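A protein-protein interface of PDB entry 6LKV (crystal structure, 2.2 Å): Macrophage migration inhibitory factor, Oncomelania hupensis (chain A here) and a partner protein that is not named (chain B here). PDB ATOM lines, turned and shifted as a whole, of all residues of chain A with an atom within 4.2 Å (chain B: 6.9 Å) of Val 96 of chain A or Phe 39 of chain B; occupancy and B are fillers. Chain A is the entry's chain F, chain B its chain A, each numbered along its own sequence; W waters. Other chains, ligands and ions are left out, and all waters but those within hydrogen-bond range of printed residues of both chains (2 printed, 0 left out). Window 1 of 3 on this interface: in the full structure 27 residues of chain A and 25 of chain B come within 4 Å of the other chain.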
ATOM      1  N   ILE A  48      13.876 -13.678   4.205  1.00  0.00           N
ATOM      2  CA  ILE A  48      14.508 -12.880   5.279  1.00  0.00           C
ATOM      3  C   ILE A  48      15.991 -12.771   4.944  1.00  0.00           C
ATOM      4  O   ILE A  48      16.613 -13.797   4.667  1.00  0.00           O
ATOM      5  CB  ILE A  48      14.228 -13.475   6.676  1.00  0.00           C
ATOM      6  CG1 ILE A  48      14.768 -12.553   7.776  1.00  0.00           C
ATOM      7  CG2 ILE A  48      14.760 -14.888   6.818  1.00  0.00           C
ATOM      8  CD1 ILE A  48      14.275 -12.916   9.161  1.00  0.00           C
ATOM      9  N   MET A  49      16.497 -11.559   4.875  1.00  0.00           N
ATOM     10  CA  MET A  49      17.940 -11.287   4.712  1.00  0.00           C
ATOM     11  C   MET A  49      18.433 -10.552   5.968  1.00  0.00           C
ATOM     12  O   MET A  49      17.610  -9.957   6.736  1.00  0.00           O
ATOM     13  CB  MET A  49      18.228 -10.453   3.464  1.00  0.00           C
ATOM     14  CG  MET A  49      17.540  -9.115   3.426  1.00  0.00           C
ATOM     15  SD  MET A  49      18.287  -7.990   2.188  1.00  0.00           S
ATOM     16  CE  MET A  49      18.082  -8.953   0.700  1.00  0.00           C
ATOM     17  N   MET A  50      19.734 -10.628   6.200  1.00  0.00           N
ATOM     18  CA  MET A  50      20.389  -9.985   7.369  1.00  0.00           C
ATOM     19  C   MET A  50      21.670  -9.314   6.873  1.00  0.00           C
ATOM     20  O   MET A  50      22.441  -9.986   6.172  1.00  0.00           O
ATOM     21  CB  MET A  50      20.691 -11.071   8.401  1.00  0.00           C
ATOM     22  CG  MET A  50      21.319 -10.549   9.688  1.00  0.00           C
ATOM     23  SD  MET A  50      21.921 -11.929  10.676  1.00  0.00           S
ATOM     24  CE  MET A  50      22.464 -11.005  12.109  1.00  0.00           C
ATOM     25  N   CYS A  57      20.426 -17.242   8.014  1.00  0.00           N
ATOM     26  CA  CYS A  57      20.171 -16.416   9.225  1.00  0.00           C
ATOM     27  C   CYS A  57      18.884 -16.891   9.919  1.00  0.00           C
ATOM     28  O   CYS A  57      18.077 -17.648   9.312  1.00  0.00           O
ATOM     29  CB  CYS A  57      20.124 -14.942   8.869  1.00  0.00           C
ATOM     30  SG  CYS A  57      18.687 -14.468   7.862  1.00  0.00           S
ATOM     31  N   VAL A  58      18.741 -16.516  11.189  1.00  0.00           N
ATOM     32  CA  VAL A  58      17.552 -16.847  12.013  1.00  0.00           C
ATOM     33  C   VAL A  58      17.190 -15.598  12.804  1.00  0.00           C
ATOM     34  O   VAL A  58      18.082 -15.052  13.516  1.00  0.00           O
ATOM     35  CB  VAL A  58      17.809 -18.014  12.980  1.00  0.00           C
ATOM     36  CG1 VAL A  58      16.575 -18.260  13.881  1.00  0.00           C
ATOM     37  CG2 VAL A  58      18.203 -19.275  12.249  1.00  0.00           C
ATOM     38  N   PHE A  59      15.938 -15.169  12.700  1.00  0.00           N
ATOM     39  CA  PHE A  59      15.318 -14.270  13.704  1.00  0.00           C
ATOM     40  C   PHE A  59      14.248 -15.090  14.390  1.00  0.00           C
ATOM     41  O   PHE A  59      13.305 -15.578  13.693  1.00  0.00           O
ATOM     42  CB  PHE A  59      14.782 -12.964  13.124  1.00  0.00           C
ATOM     43  CG  PHE A  59      14.014 -12.150  14.146  1.00  0.00           C
ATOM     44  CD1 PHE A  59      14.603 -11.813  15.347  1.00  0.00           C
ATOM     45  CD2 PHE A  59      12.691 -11.805  13.958  1.00  0.00           C
ATOM     46  CE1 PHE A  59      13.916 -11.084  16.307  1.00  0.00           C
ATOM     47  CE2 PHE A  59      11.994 -11.083  14.924  1.00  0.00           C
ATOM     48  CZ  PHE A  59      12.613 -10.705  16.093  1.00  0.00           C
ATOM     49  N   ALA A  60      14.408 -15.313  15.700  1.00  0.00           N
ATOM     50  CA  ALA A  60      13.440 -16.108  16.479  1.00  0.00           C
ATOM     51  C   ALA A  60      12.858 -15.273  17.617  1.00  0.00           C
ATOM     52  O   ALA A  60      13.542 -14.400  18.128  1.00  0.00           O
ATOM     53  CB  ALA A  60      14.120 -17.362  16.983  1.00  0.00           C
ATOM     54  N   ILE A  95      22.319 -15.065  14.114  1.00  0.00           N
ATOM     55  CA  ILE A  95      21.144 -15.416  14.961  1.00  0.00           C
ATOM     56  C   ILE A  95      20.828 -14.258  15.914  1.00  0.00           C
ATOM     57  O   ILE A  95      21.729 -13.813  16.685  1.00  0.00           O
ATOM     58  CB  ILE A  95      21.385 -16.718  15.728  1.00  0.00           C
ATOM     59  CG1 ILE A  95      21.762 -17.868  14.794  1.00  0.00           C
ATOM     60  CG2 ILE A  95      20.180 -17.047  16.595  1.00  0.00           C
ATOM     61  CD1 ILE A  95      22.233 -19.103  15.527  1.00  0.00           C
ATOM     62  N   VAL A  96      19.572 -13.816  15.877  1.00  0.00           N
ATOM     63  CA  VAL A  96      18.987 -12.854  16.847  1.00  0.00           C
ATOM     64  C   VAL A  96      17.714 -13.491  17.387  1.00  0.00           C
ATOM     65  O   VAL A  96      16.940 -14.057  16.591  1.00  0.00           O
ATOM     66  CB  VAL A  96      18.742 -11.477  16.210  1.00  0.00           C
ATOM     67  CG1 VAL A  96      17.856 -10.584  17.078  1.00  0.00           C
ATOM     68  CG2 VAL A  96      20.043 -10.783  15.879  1.00  0.00           C
ATOM     69  N   ILE A  97      17.565 -13.469  18.704  1.00  0.00           N
ATOM     70  CA  ILE A  97      16.376 -13.994  19.421  1.00  0.00           C
ATOM     71  C   ILE A  97      15.829 -12.861  20.280  1.00  0.00           C
ATOM     72  O   ILE A  97      16.612 -12.205  21.006  1.00  0.00           O
ATOM     73  CB  ILE A  97      16.721 -15.226  20.266  1.00  0.00           C
ATOM     74  CG1 ILE A  97      17.456 -16.285  19.442  1.00  0.00           C
ATOM     75  CG2 ILE A  97      15.462 -15.764  20.930  1.00  0.00           C
ATOM     76  CD1 ILE A  97      18.091 -17.375  20.315  1.00  0.00           C
ATOM     77  N   MET B   1      16.368  -7.796  16.822  1.00  0.00           N
ATOM     78  CA  MET B   1      16.418  -6.401  16.419  1.00  0.00           C
ATOM     79  C   MET B   1      17.756  -6.062  15.729  1.00  0.00           C
ATOM     80  O   MET B   1      18.769  -6.753  15.948  1.00  0.00           O
ATOM     81  CB  MET B   1      16.190  -5.553  17.674  1.00  0.00           C
ATOM     82  CG  MET B   1      17.486  -5.098  18.301  1.00  0.00           C
ATOM     83  SD  MET B   1      18.208  -3.632  17.525  1.00  0.00           S
ATOM     84  CE  MET B   1      19.939  -3.927  17.934  1.00  0.00           C
ATOM     85  N   PRO B   2      17.825  -5.019  14.837  1.00  0.00           N
ATOM     86  CA  PRO B   2      16.648  -4.364  14.287  1.00  0.00           C
ATOM     87  C   PRO B   2      16.106  -5.368  13.257  1.00  0.00           C
ATOM     88  O   PRO B   2      16.871  -6.033  12.549  1.00  0.00           O
ATOM     89  CB  PRO B   2      17.114  -3.021  13.716  1.00  0.00           C
ATOM     90  CG  PRO B   2      18.594  -2.976  14.032  1.00  0.00           C
ATOM     91  CD  PRO B   2      19.024  -4.396  14.307  1.00  0.00           C
ATOM     92  N   VAL B   3      14.808  -5.574  13.318  1.00  0.00           N
ATOM     93  CA  VAL B   3      14.084  -6.452  12.370  1.00  0.00           C
ATOM     94  C   VAL B   3      12.973  -5.612  11.776  1.00  0.00           C
ATOM     95  O   VAL B   3      12.163  -5.074  12.579  1.00  0.00           O
ATOM     96  CB  VAL B   3      13.544  -7.691  13.090  1.00  0.00           C
ATOM     97  CG1 VAL B   3      12.815  -8.598  12.115  1.00  0.00           C
ATOM     98  CG2 VAL B   3      14.653  -8.426  13.822  1.00  0.00           C
ATOM     99  N   ILE B   4      12.988  -5.467  10.457  1.00  0.00           N
ATOM    100  CA  ILE B   4      11.911  -4.808   9.666  1.00  0.00           C
ATOM    101  C   ILE B   4      11.112  -5.945   9.031  1.00  0.00           C
ATOM    102  O   ILE B   4      11.710  -6.724   8.234  1.00  0.00           O
ATOM    103  CB  ILE B   4      12.474  -3.866   8.603  1.00  0.00           C
ATOM    104  CG1 ILE B   4      13.722  -3.089   9.055  1.00  0.00           C
ATOM    105  CG2 ILE B   4      11.377  -2.954   8.068  1.00  0.00           C
ATOM    106  CD1 ILE B   4      13.551  -2.246  10.260  1.00  0.00           C
ATOM    107  N   THR B   5       9.846  -6.098   9.409  1.00  0.00           N
ATOM    108  CA  THR B   5       8.942  -7.128   8.840  1.00  0.00           C
ATOM    109  C   THR B   5       7.938  -6.406   7.956  1.00  0.00           C
ATOM    110  O   THR B   5       7.271  -5.476   8.440  1.00  0.00           O
ATOM    111  CB  THR B   5       8.310  -7.988   9.940  1.00  0.00           C
ATOM    112  OG1 THR B   5       9.375  -8.511  10.741  1.00  0.00           O
ATOM    113  CG2 THR B   5       7.531  -9.168   9.413  1.00  0.00           C
ATOM    114  N   THR B  24      16.950  -2.150   3.802  1.00  0.00           N
ATOM    115  CA  THR B  24      18.085  -2.414   4.710  1.00  0.00           C
ATOM    116  C   THR B  24      18.927  -1.135   4.821  1.00  0.00           C
ATOM    117  O   THR B  24      19.125  -0.635   5.950  1.00  0.00           O
ATOM    118  CB  THR B  24      18.949  -3.584   4.246  1.00  0.00           C
ATOM    119  OG1 THR B  24      18.204  -4.800   4.214  1.00  0.00           O
ATOM    120  CG2 THR B  24      20.158  -3.771   5.140  1.00  0.00           C
ATOM    121  N   LYS B  35      24.808  -2.337  10.019  1.00  0.00           N
ATOM    122  CA  LYS B  35      24.104  -2.991   8.895  1.00  0.00           C
ATOM    123  C   LYS B  35      24.042  -4.501   9.155  1.00  0.00           C
ATOM    124  O   LYS B  35      23.018  -5.103   8.829  1.00  0.00           O
ATOM    125  CB  LYS B  35      24.804  -2.668   7.575  1.00  0.00           C
ATOM    126  CG  LYS B  35      24.086  -3.218   6.341  1.00  0.00           C
ATOM    127  CD  LYS B  35      24.463  -2.559   5.039  1.00  0.00           C
ATOM    128  CE  LYS B  35      24.223  -3.483   3.866  1.00  0.00           C
ATOM    129  NZ  LYS B  35      24.259  -2.741   2.588  1.00  0.00           N
ATOM    130  N   GLU B  36      25.089  -5.059   9.759  1.00  0.00           N
ATOM    131  CA  GLU B  36      25.306  -6.508   9.968  1.00  0.00           C
ATOM    132  C   GLU B  36      24.105  -7.153  10.670  1.00  0.00           C
ATOM    133  O   GLU B  36      23.865  -8.338  10.407  1.00  0.00           O
ATOM    134  CB  GLU B  36      26.582  -6.755  10.783  1.00  0.00           C
ATOM    135  CG  GLU B  36      27.865  -6.527   9.980  1.00  0.00           C
ATOM    136  CD  GLU B  36      28.260  -5.077   9.693  1.00  0.00           C
ATOM    137  OE1 GLU B  36      27.769  -4.137  10.398  1.00  0.00           O
ATOM    138  OE2 GLU B  36      29.041  -4.876   8.732  1.00  0.00           O
ATOM    139  N   VAL B  37      23.440  -6.437  11.581  1.00  0.00           N
ATOM    140  CA  VAL B  37      22.333  -7.009  12.410  1.00  0.00           C
ATOM    141  C   VAL B  37      20.974  -6.477  11.924  1.00  0.00           C
ATOM    142  O   VAL B  37      20.009  -6.672  12.616  1.00  0.00           O
ATOM    143  CB  VAL B  37      22.566  -6.765  13.922  1.00  0.00           C
ATOM    144  CG1 VAL B  37      23.866  -7.420  14.379  1.00  0.00           C
ATOM    145  CG2 VAL B  37      22.552  -5.286  14.278  1.00  0.00           C
ATOM    146  N   MET B  38      20.906  -5.828  10.775  1.00  0.00           N
ATOM    147  CA  MET B  38      19.608  -5.361  10.209  1.00  0.00           C
ATOM    148  C   MET B  38      18.978  -6.524   9.423  1.00  0.00           C
ATOM    149  O   MET B  38      19.517  -6.938   8.396  1.00  0.00           O
ATOM    150  CB  MET B  38      19.810  -4.164   9.280  1.00  0.00           C
ATOM    151  CG  MET B  38      18.509  -3.574   8.735  1.00  0.00           C
ATOM    152  SD  MET B  38      17.604  -2.552   9.908  1.00  0.00           S
ATOM    153  CE  MET B  38      18.935  -1.697  10.748  1.00  0.00           C
ATOM    154  N   PHE B  39      17.858  -7.027   9.908  1.00  0.00           N
ATOM    155  CA  PHE B  39      17.026  -8.025   9.204  1.00  0.00           C
ATOM    156  C   PHE B  39      15.927  -7.293   8.448  1.00  0.00           C
ATOM    157  O   PHE B  39      15.341  -6.359   9.036  1.00  0.00           O
ATOM    158  CB  PHE B  39      16.331  -8.964  10.167  1.00  0.00           C
ATOM    159  CG  PHE B  39      17.223  -9.969  10.837  1.00  0.00           C
ATOM    160  CD1 PHE B  39      17.928  -9.628  11.987  1.00  0.00           C
ATOM    161  CD2 PHE B  39      17.270 -11.273  10.383  1.00  0.00           C
ATOM    162  CE1 PHE B  39      18.696 -10.575  12.643  1.00  0.00           C
ATOM    163  CE2 PHE B  39      18.055 -12.220  11.034  1.00  0.00           C
ATOM    164  CZ  PHE B  39      18.768 -11.863  12.158  1.00  0.00           C
ATOM    165  N   VAL B  40      15.656  -7.724   7.211  1.00  0.00           N
ATOM    166  CA  VAL B  40      14.390  -7.400   6.510  1.00  0.00           C
ATOM    167  C   VAL B  40      13.717  -8.712   6.114  1.00  0.00           C
ATOM    168  O   VAL B  40      14.303  -9.510   5.307  1.00  0.00           O
ATOM    169  CB  VAL B  40      14.606  -6.467   5.315  1.00  0.00           C
ATOM    170  CG1 VAL B  40      13.284  -6.121   4.671  1.00  0.00           C
ATOM    171  CG2 VAL B  40      15.377  -5.215   5.712  1.00  0.00           C
ATOM    172  N   ASP B  41      12.538  -8.934   6.687  1.00  0.00           N
ATOM    173  CA  ASP B  41      11.702 -10.132   6.445  1.00  0.00           C
ATOM    174  C   ASP B  41      10.533  -9.673   5.589  1.00  0.00           C
ATOM    175  O   ASP B  41       9.636  -9.006   6.134  1.00  0.00           O
ATOM    176  CB  ASP B  41      11.248 -10.773   7.755  1.00  0.00           C
ATOM    177  CG  ASP B  41      10.553 -12.114   7.585  1.00  0.00           C
ATOM    178  OD1 ASP B  41      10.374 -12.557   6.434  1.00  0.00           O
ATOM    179  OD2 ASP B  41      10.219 -12.722   8.611  1.00  0.00           O
ATOM    180  N   CYS B 107      16.916  -9.553  24.342  1.00  0.00           N
ATOM    181  CA  CYS B 107      17.338  -9.749  22.945  1.00  0.00           C
ATOM    182  C   CYS B 107      18.794 -10.219  22.894  1.00  0.00           C
ATOM    183  O   CYS B 107      19.691  -9.454  23.365  1.00  0.00           O
ATOM    184  CB  CYS B 107      17.139  -8.474  22.144  1.00  0.00           C
ATOM    185  SG  CYS B 107      17.418  -8.744  20.373  1.00  0.00           S
ATOM    186  N   SER B 108      19.012 -11.408  22.319  1.00  0.00           N
ATOM    187  CA  SER B 108      20.355 -12.004  22.076  1.00  0.00           C
ATOM    188  C   SER B 108      20.850 -11.737  20.647  1.00  0.00           C
ATOM    189  O   SER B 108      20.026 -11.700  19.705  1.00  0.00           O
ATOM    190  CB  SER B 108      20.368 -13.464  22.386  1.00  0.00           C
ATOM    191  OG  SER B 108      19.491 -14.195  21.551  1.00  0.00           O
ATOM    192  N   PHE B 109      22.153 -11.504  20.511  1.00  0.00           N
ATOM    193  CA  PHE B 109      22.910 -11.593  19.250  1.00  0.00           C
ATOM    194  C   PHE B 109      24.246 -12.274  19.548  1.00  0.00           C
ATOM    195  O   PHE B 109      24.943 -11.832  20.489  1.00  0.00           O
ATOM    196  CB  PHE B 109      23.126 -10.201  18.657  1.00  0.00           C
ATOM    197  CG  PHE B 109      24.141 -10.188  17.551  1.00  0.00           C
ATOM    198  CD1 PHE B 109      23.975 -11.003  16.435  1.00  0.00           C
ATOM    199  CD2 PHE B 109      25.282  -9.409  17.644  1.00  0.00           C
ATOM    200  CE1 PHE B 109      24.909 -10.999  15.409  1.00  0.00           C
ATOM    201  CE2 PHE B 109      26.229  -9.412  16.619  1.00  0.00           C
ATOM    202  CZ  PHE B 109      26.036 -10.202  15.505  1.00  0.00           C
ATOM    203  N   ASN B 110      24.602 -13.299  18.782  1.00  0.00           N
ATOM    204  CA  ASN B 110      25.971 -13.855  18.761  1.00  0.00           C
ATOM    205  C   ASN B 110      26.407 -14.236  20.189  1.00  0.00           C
ATOM    206  O   ASN B 110      27.504 -13.897  20.571  1.00  0.00           O
ATOM    207  CB  ASN B 110      26.969 -12.869  18.147  1.00  0.00           C
ATOM    208  CG  ASN B 110      28.308 -13.530  17.791  1.00  0.00           C
ATOM    209  OD1 ASN B 110      28.413 -14.755  17.602  1.00  0.00           O
ATOM    210  ND2 ASN B 110      29.349 -12.724  17.700  1.00  0.00           N
ATOM    211  N   HIS B 114      22.336  -7.589  24.994  1.00  0.00           N
ATOM    212  CA  HIS B 114      22.795  -6.255  24.560  1.00  0.00           C
ATOM    213  C   HIS B 114      23.011  -5.383  25.795  1.00  0.00           C
ATOM    214  O   HIS B 114      22.420  -5.653  26.844  1.00  0.00           O
ATOM    215  CB  HIS B 114      21.787  -5.641  23.572  1.00  0.00           C
ATOM    216  CG  HIS B 114      21.724  -6.342  22.259  1.00  0.00           C
ATOM    217  ND1 HIS B 114      21.037  -7.539  22.094  1.00  0.00           N
ATOM    218  CD2 HIS B 114      22.219  -6.005  21.050  1.00  0.00           C
ATOM    219  CE1 HIS B 114      21.142  -7.921  20.831  1.00  0.00           C
ATOM    220  NE2 HIS B 114      21.858  -6.981  20.170  1.00  0.00           N
HETATM  221  O   HOH W   1      19.081  -7.076   5.602  1.00  0.00           O
HETATM  222  O   HOH W   2      21.026 -14.798  19.409  1.00  0.00           O
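Among the printed residues, pairs that only touch across the chains: Ile 48 of chain A with Phe 39 of chain B, Ile 48 of chain A with Val 40 of chain B, Ile 48 of chain A with Asp 41 of chain B, Met 49 of chain A with Met 38 of chain B, Met 49 of chain A with Phe 39 of chain B, Met 50 of chain A with Glu 36 of chain B, Met 50 of chain A with Met 38 of chain B, Met 50 of chain A with Phe 39 of chain B, Cys 57 of chain A with Phe 39 of chain B, Val 58 of chain A with Phe 39 of chain B, Phe 59 of chain A with Val 3 of chain B, Phe 59 of chain A with Phe 39 of chain B, Ile 95 of chain A with Phe 109 of chain B, Ile 95 of chain A with Asn 110 of chain B, Val 96 of chain A with Met 1 of chain B, Val 96 of chain A with Phe 39 of chain B, Val 96 of chain A with Cys 107 of chain B, Val 96 of chain A with Ser 108 of chain B and Val 96 of chain A with Phe 109 of chain B.
The backbone carbonyl oxygen (O) of Val 58 of chain A is in hydrogen-bond range of the backbone NH (N) of Val 96 of chain A (3.1 Å).
The backbone carbonyl oxygen (O) of Cys 107 of chain B sits at hydrogen-bond distance from a ring nitrogen (ND1) of His 114 of chain B, at 2.7 Å.
The backbone carbonyl oxygen of Pro 2 of chain B is in hydrogen-bond range of the backbone NH of Phe 39 of chain B (3.0 Å).
N of Ile 4 of chain B lies within hydrogen-bond range of O of Phe 39 of chain B (2.9 Å).
O of Ile 4 of chain B is in hydrogen-bond range of N of Asp 41 of chain B (2.8 Å).
O of Val 96 of chain A lies within hydrogen-bond range of N of Ala 60 of chain A (3.0 Å).
Of the 18 printed residues of chain B, 12 touch a printed residue of chain A.
Printed residues of chain B that touch a printed residue of chain A: Met 1, Val 3, Thr 24, Glu 36, Met 38, Phe 39, Val 40, Asp 41, Cys 107, Ser 108, Phe 109 and Asn 110.
Of the 10 printed residues of chain A, 9 touch a printed residue of chain B.
Hydrophobic or aromatic side chains of chain A that line the printed part of chain B: Ile 48, Met 49, Met 50, Phe 59, Val 96 and Ile 97.
Val 96 of chain A touches just these residues of chain B: Met 1 (3.2 Å), Phe 39 (3.5 Å), Cys 107 (3.8 Å), Ser 108 (3.3 Å) and Phe 109 (3.98 Å).
Phe 39 of chain B touches just these residues of chain A: Ile 48 (3.6 Å), Met 49 (3.2 Å), Met 50 (3.5 Å), Cys 57 (3.9 Å), Val 58 (3.5 Å), Phe 59 (3.95 Å) and Val 96 (3.5 Å).
Printed residues of chain A within 4 Å of Met 1 of chain B: Val 96.
Of the printed residues of chain A, Cys 107 of chain B touches Val 96 (3.8 Å) and Ile 97 (3.2 Å).
Of the printed residues of chain A, Ser 108 of chain B touches Val 96 and Ile 97.
His 114 of chain B touches none of the printed residues of chain A.
The nearest residue of chain B that does not touch Val 96 of chain A is Val 3 of chain B (5.1 Å).
The nearest printed residue of chain A that does not touch Phe 39 of chain B is Ile 95 of chain A (4.9 Å).
Water W2 lies within hydrogen-bond range of OG of Ser 108 of chain B (2.7 Å) and O of Ile 95 of chain A (3.0 Å).
Water W1 lies within hydrogen-bond range of OG1 of Thr 24 of chain B (2.8 Å), O of Met 38 of chain B (2.8 Å) and O of Met 49 of chain A (3.4 Å).
The backbone carbonyl oxygen (O) of Met 49 of chain A lies within hydrogen-bond range of the backbone NH (N) of Val 40 of chain B (3.0 Å).
O of Ile 97 of chain A lies close to SG of Cys 107 of chain B (3.6 Å).
The backbone carbonyl oxygen (O) of Ile 97 of chain A sits at hydrogen-bond distance from the backbone NH (N) of Ser 108 of chain B, 2.8 Å away.
The side-chain sulfur of Met 49 of chain A lies within hydrogen-bond range of the side-chain hydroxyl of Thr 24 of chain B (3.8 Å).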
